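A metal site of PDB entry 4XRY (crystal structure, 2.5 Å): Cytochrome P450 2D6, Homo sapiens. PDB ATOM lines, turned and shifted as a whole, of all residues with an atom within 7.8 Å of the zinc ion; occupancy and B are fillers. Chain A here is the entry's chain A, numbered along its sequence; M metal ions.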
ATOM      1  N   ALA A 165       3.026   3.862 -24.747  1.00  0.00           N
ATOM      2  CA  ALA A 165       2.226   4.873 -24.060  1.00  0.00           C
ATOM      3  C   ALA A 165       0.879   5.042 -24.746  1.00  0.00           C
ATOM      4  O   ALA A 165      -0.140   5.259 -24.087  1.00  0.00           O
ATOM      5  CB  ALA A 165       2.969   6.197 -24.028  1.00  0.00           C
ATOM      6  N   SER A 166       0.873   4.936 -26.069  1.00  0.00           N
ATOM      7  CA  SER A 166      -0.357   5.054 -26.848  1.00  0.00           C
ATOM      8  C   SER A 166      -1.298   3.894 -26.554  1.00  0.00           C
ATOM      9  O   SER A 166      -2.510   4.056 -26.525  1.00  0.00           O
ATOM     10  CB  SER A 166      -0.036   5.101 -28.336  1.00  0.00           C
ATOM     11  OG  SER A 166       0.964   6.073 -28.598  1.00  0.00           O
ATOM     12  N   LEU A 167      -0.725   2.712 -26.356  1.00  0.00           N
ATOM     13  CA  LEU A 167      -1.521   1.533 -26.073  1.00  0.00           C
ATOM     14  C   LEU A 167      -1.989   1.524 -24.630  1.00  0.00           C
ATOM     15  O   LEU A 167      -3.138   1.209 -24.343  1.00  0.00           O
ATOM     16  CB  LEU A 167      -0.739   0.257 -26.398  1.00  0.00           C
ATOM     17  CG  LEU A 167      -0.412   0.115 -27.877  1.00  0.00           C
ATOM     18  CD1 LEU A 167       0.032  -1.288 -28.219  1.00  0.00           C
ATOM     19  CD2 LEU A 167      -1.624   0.503 -28.705  1.00  0.00           C
ATOM     20  N   THR A 168      -1.080   1.867 -23.716  1.00  0.00           N
ATOM     21  CA  THR A 168      -1.405   1.879 -22.298  1.00  0.00           C
ATOM     22  C   THR A 168      -2.255   3.090 -21.917  1.00  0.00           C
ATOM     23  O   THR A 168      -3.364   2.929 -21.405  1.00  0.00           O
ATOM     24  CB  THR A 168      -0.134   1.832 -21.435  1.00  0.00           C
ATOM     25  OG1 THR A 168       0.828   2.772 -21.938  1.00  0.00           O
ATOM     26  CG2 THR A 168       0.487   0.447 -21.480  1.00  0.00           C
ATOM     27  N   CYS A 169      -1.750   4.298 -22.167  1.00  0.00           N
ATOM     28  CA  CYS A 169      -2.436   5.498 -21.687  1.00  0.00           C
ATOM     29  C   CYS A 169      -3.117   6.324 -22.782  1.00  0.00           C
ATOM     30  O   CYS A 169      -3.691   7.368 -22.499  1.00  0.00           O
ATOM     31  CB  CYS A 169      -1.452   6.381 -20.919  1.00  0.00           C
ATOM     32  SG  CYS A 169      -1.122   5.794 -19.242  1.00  0.00           S
ATOM     33  N   GLY A 170      -3.059   5.860 -24.022  1.00  0.00           N
ATOM     34  CA  GLY A 170      -3.753   6.534 -25.105  1.00  0.00           C
ATOM     35  C   GLY A 170      -3.222   7.915 -25.450  1.00  0.00           C
ATOM     36  O   GLY A 170      -3.958   8.771 -25.935  1.00  0.00           O
ATOM     37  N   ARG A 171      -1.936   8.144 -25.197  1.00  0.00           N
ATOM     38  CA  ARG A 171      -1.317   9.413 -25.563  1.00  0.00           C
ATOM     39  C   ARG A 171       0.125   9.183 -26.018  1.00  0.00           C
ATOM     40  O   ARG A 171       0.684   8.113 -25.806  1.00  0.00           O
ATOM     41  CB  ARG A 171      -1.340  10.390 -24.396  1.00  0.00           C
ATOM     42  CG  ARG A 171      -0.311  10.084 -23.313  1.00  0.00           C
ATOM     43  CD  ARG A 171      -0.025  11.288 -22.432  1.00  0.00           C
ATOM     44  NE  ARG A 171       0.600  12.369 -23.177  1.00  0.00           N
ATOM     45  CZ  ARG A 171       1.037  13.504 -22.626  1.00  0.00           C
ATOM     46  NH1 ARG A 171       0.929  13.688 -21.323  1.00  0.00           N
ATOM     47  NH2 ARG A 171       1.598  14.440 -23.384  1.00  0.00           N
ATOM     48  N   HIS A 236      -4.218  10.295 -16.060  1.00  0.00           N
ATOM     49  CA  HIS A 236      -4.998   9.493 -16.991  1.00  0.00           C
ATOM     50  C   HIS A 236      -6.358   9.121 -16.391  1.00  0.00           C
ATOM     51  O   HIS A 236      -7.360   9.071 -17.087  1.00  0.00           O
ATOM     52  CB  HIS A 236      -4.226   8.235 -17.391  1.00  0.00           C
ATOM     53  CG  HIS A 236      -4.849   7.485 -18.528  1.00  0.00           C
ATOM     54  ND1 HIS A 236      -4.493   6.194 -18.849  1.00  0.00           N
ATOM     55  CD2 HIS A 236      -5.795   7.842 -19.423  1.00  0.00           C
ATOM     56  CE1 HIS A 236      -5.199   5.792 -19.888  1.00  0.00           C
ATOM     57  NE2 HIS A 236      -5.997   6.774 -20.256  1.00  0.00           N
ATOM     58  N   ARG A 237      -6.367   8.868 -15.085  1.00  0.00           N
ATOM     59  CA  ARG A 237      -7.590   8.503 -14.387  1.00  0.00           C
ATOM     60  C   ARG A 237      -8.559   9.690 -14.356  1.00  0.00           C
ATOM     61  O   ARG A 237      -9.775   9.511 -14.297  1.00  0.00           O
ATOM     62  CB  ARG A 237      -7.287   8.027 -12.960  1.00  0.00           C
ATOM     63  CG  ARG A 237      -8.453   7.316 -12.276  1.00  0.00           C
ATOM     64  CD  ARG A 237      -8.139   7.058 -10.803  1.00  0.00           C
ATOM     65  NE  ARG A 237      -7.109   6.053 -10.609  1.00  0.00           N
ATOM     66  CZ  ARG A 237      -7.359   4.787 -10.268  1.00  0.00           C
ATOM     67  NH1 ARG A 237      -8.609   4.389 -10.094  1.00  0.00           N
ATOM     68  NH2 ARG A 237      -6.356   3.930 -10.102  1.00  0.00           N
ATOM     69  N   THR A 239      -8.789  12.043 -16.872  1.00  0.00           N
ATOM     70  CA  THR A 239      -9.329  12.306 -18.203  1.00  0.00           C
ATOM     71  C   THR A 239     -10.166  11.143 -18.726  1.00  0.00           C
ATOM     72  O   THR A 239     -10.844  11.275 -19.752  1.00  0.00           O
ATOM     73  CB  THR A 239      -8.205  12.583 -19.231  1.00  0.00           C
ATOM     74  OG1 THR A 239      -7.323  11.466 -19.290  1.00  0.00           O
ATOM     75  CG2 THR A 239      -7.418  13.836 -18.840  1.00  0.00           C
ATOM     76  N   TRP A 240     -10.123  10.016 -18.028  1.00  0.00           N
ATOM     77  CA  TRP A 240     -10.838   8.803 -18.440  1.00  0.00           C
ATOM     78  C   TRP A 240     -12.353   9.011 -18.462  1.00  0.00           C
ATOM     79  O   TRP A 240     -12.945   9.424 -17.463  1.00  0.00           O
ATOM     80  CB  TRP A 240     -10.494   7.639 -17.510  1.00  0.00           C
ATOM     81  CG  TRP A 240     -11.327   6.412 -17.735  1.00  0.00           C
ATOM     82  CD1 TRP A 240     -11.757   5.905 -18.933  1.00  0.00           C
ATOM     83  CD2 TRP A 240     -11.865   5.546 -16.725  1.00  0.00           C
ATOM     84  NE1 TRP A 240     -12.508   4.772 -18.726  1.00  0.00           N
ATOM     85  CE2 TRP A 240     -12.597   4.538 -17.381  1.00  0.00           C
ATOM     86  CE3 TRP A 240     -11.804   5.539 -15.325  1.00  0.00           C
ATOM     87  CZ2 TRP A 240     -13.252   3.518 -16.686  1.00  0.00           C
ATOM     88  CZ3 TRP A 240     -12.451   4.524 -14.643  1.00  0.00           C
ATOM     89  CH2 TRP A 240     -13.163   3.528 -15.319  1.00  0.00           C
ATOM     90  N   ASP A 241     -12.961   8.710 -19.605  1.00  0.00           N
ATOM     91  CA  ASP A 241     -14.409   8.797 -19.768  1.00  0.00           C
ATOM     92  C   ASP A 241     -15.023   7.402 -19.777  1.00  0.00           C
ATOM     93  O   ASP A 241     -15.029   6.727 -20.806  1.00  0.00           O
ATOM     94  CB  ASP A 241     -14.755   9.558 -21.049  1.00  0.00           C
ATOM     95  CG  ASP A 241     -16.252   9.758 -21.239  1.00  0.00           C
ATOM     96  OD1 ASP A 241     -16.661  10.197 -22.329  1.00  0.00           O
ATOM     97  OD2 ASP A 241     -17.025   9.464 -20.302  1.00  0.00           O
ATOM     98  N   PRO A 246     -13.479   1.740 -23.593  1.00  0.00           N
ATOM     99  CA  PRO A 246     -12.069   1.932 -23.265  1.00  0.00           C
ATOM    100  C   PRO A 246     -11.229   2.238 -24.499  1.00  0.00           C
ATOM    101  O   PRO A 246     -11.333   1.549 -25.510  1.00  0.00           O
ATOM    102  CB  PRO A 246     -11.659   0.597 -22.653  1.00  0.00           C
ATOM    103  CG  PRO A 246     -12.920   0.112 -22.012  1.00  0.00           C
ATOM    104  CD  PRO A 246     -14.048   0.573 -22.892  1.00  0.00           C
ATOM    105  N   ARG A 247     -10.429   3.292 -24.424  1.00  0.00           N
ATOM    106  CA  ARG A 247      -9.666   3.751 -25.581  1.00  0.00           C
ATOM    107  C   ARG A 247      -8.237   3.218 -25.553  1.00  0.00           C
ATOM    108  O   ARG A 247      -7.512   3.291 -26.542  1.00  0.00           O
ATOM    109  CB  ARG A 247      -9.667   5.284 -25.620  1.00  0.00           C
ATOM    110  CG  ARG A 247      -9.697   5.876 -27.014  1.00  0.00           C
ATOM    111  CD  ARG A 247      -9.624   7.391 -26.950  1.00  0.00           C
ATOM    112  NE  ARG A 247      -8.463   7.824 -26.198  1.00  0.00           N
ATOM    113  CZ  ARG A 247      -7.272   8.062 -26.740  1.00  0.00           C
ATOM    114  NH1 ARG A 247      -7.087   7.911 -28.044  1.00  0.00           N
ATOM    115  NH2 ARG A 247      -6.266   8.453 -25.977  1.00  0.00           N
ATOM    116  N   ASP A 248      -7.846   2.668 -24.410  1.00  0.00           N
ATOM    117  CA  ASP A 248      -6.494   2.174 -24.195  1.00  0.00           C
ATOM    118  C   ASP A 248      -6.489   1.137 -23.084  1.00  0.00           C
ATOM    119  O   ASP A 248      -7.497   0.957 -22.393  1.00  0.00           O
ATOM    120  CB  ASP A 248      -5.550   3.339 -23.877  1.00  0.00           C
ATOM    121  CG  ASP A 248      -6.109   4.267 -22.799  1.00  0.00           C
ATOM    122  OD1 ASP A 248      -6.380   3.789 -21.679  1.00  0.00           O
ATOM    123  OD2 ASP A 248      -6.270   5.472 -23.082  1.00  0.00           O
ATOM    124  N   LEU A 249      -5.368   0.444 -22.897  1.00  0.00           N
ATOM    125  CA  LEU A 249      -5.310  -0.679 -21.968  1.00  0.00           C
ATOM    126  C   LEU A 249      -5.571  -0.267 -20.525  1.00  0.00           C
ATOM    127  O   LEU A 249      -6.208  -0.994 -19.773  1.00  0.00           O
ATOM    128  CB  LEU A 249      -3.953  -1.391 -22.074  1.00  0.00           C
ATOM    129  CG  LEU A 249      -3.793  -2.633 -21.182  1.00  0.00           C
ATOM    130  CD1 LEU A 249      -3.222  -3.796 -21.968  1.00  0.00           C
ATOM    131  CD2 LEU A 249      -2.928  -2.340 -19.965  1.00  0.00           C
ATOM    132  N   THR A 250      -5.080   0.912 -20.151  1.00  0.00           N
ATOM    133  CA  THR A 250      -5.274   1.406 -18.786  1.00  0.00           C
ATOM    134  C   THR A 250      -6.757   1.652 -18.501  1.00  0.00           C
ATOM    135  O   THR A 250      -7.232   1.372 -17.390  1.00  0.00           O
ATOM    136  CB  THR A 250      -4.468   2.706 -18.548  1.00  0.00           C
ATOM    137  OG1 THR A 250      -3.067   2.401 -18.568  1.00  0.00           O
ATOM    138  CG2 THR A 250      -4.823   3.333 -17.201  1.00  0.00           C
ATOM    139  N   GLU A 251      -7.498   2.148 -19.481  1.00  0.00           N
ATOM    140  CA  GLU A 251      -8.930   2.367 -19.309  1.00  0.00           C
ATOM    141  C   GLU A 251      -9.644   1.029 -19.179  1.00  0.00           C
ATOM    142  O   GLU A 251     -10.550   0.874 -18.347  1.00  0.00           O
ATOM    143  CB  GLU A 251      -9.505   3.173 -20.464  1.00  0.00           C
ATOM    144  CG  GLU A 251      -9.097   4.644 -20.449  1.00  0.00           C
ATOM    145  CD  GLU A 251      -9.648   5.417 -21.631  1.00  0.00           C
ATOM    146  OE1 GLU A 251     -10.608   4.927 -22.260  1.00  0.00           O
ATOM    147  OE2 GLU A 251      -9.113   6.500 -21.932  1.00  0.00           O
ATOM    148  N   ALA A 252      -9.241   0.060 -19.998  1.00  0.00           N
ATOM    149  CA  ALA A 252      -9.798  -1.279 -19.928  1.00  0.00           C
ATOM    150  C   ALA A 252      -9.538  -1.893 -18.555  1.00  0.00           C
ATOM    151  O   ALA A 252     -10.401  -2.556 -17.971  1.00  0.00           O
ATOM    152  CB  ALA A 252      -9.218  -2.162 -21.019  1.00  0.00           C
ATOM    153  N   LEU A 254      -9.002  -0.155 -15.741  1.00  0.00           N
ATOM    154  CA  LEU A 254      -9.786   0.599 -14.761  1.00  0.00           C
ATOM    155  C   LEU A 254     -11.246   0.159 -14.738  1.00  0.00           C
ATOM    156  O   LEU A 254     -11.864   0.096 -13.673  1.00  0.00           O
ATOM    157  CB  LEU A 254      -9.692   2.106 -15.048  1.00  0.00           C
ATOM    158  CG  LEU A 254      -8.340   2.779 -14.808  1.00  0.00           C
ATOM    159  CD1 LEU A 254      -8.281   4.135 -15.496  1.00  0.00           C
ATOM    160  CD2 LEU A 254      -8.044   2.919 -13.321  1.00  0.00           C
HETATM  161 ZN    ZN M   1      -7.199   6.825 -21.944  1.00  0.00          ZN
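The side-chain carboxylate of Glu 251 lies within hydrogen-bond range of the backbone NH of Arg 247, at 2.7 Å. The side-chain carboxylate of Asp 248 lies close to the backbone NH of Gly 170. A ring nitrogen (NE2) of His 236 lies close to the backbone carbonyl oxygen of Cys 169, 3.3 Å away. The backbone carbonyl oxygen (O) of His 236 is in hydrogen-bond range of the side-chain hydroxyl (OG1) of Thr 239, at 3.3 Å.
Merely in contact with the zinc ion: Cys 169. Four residues have an atom within 4 Å of the zinc ion: Cys 169, His 236, Asp 248 and Glu 251.
The zinc ion is bound by OE2 of Glu 251. OD2 of Asp 248 binds the zinc ion. The zinc ion is bound by a ring nitrogen (NE2) of His 236, 2.1 Å away. The zinc ion has three donor atoms within binding distance.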
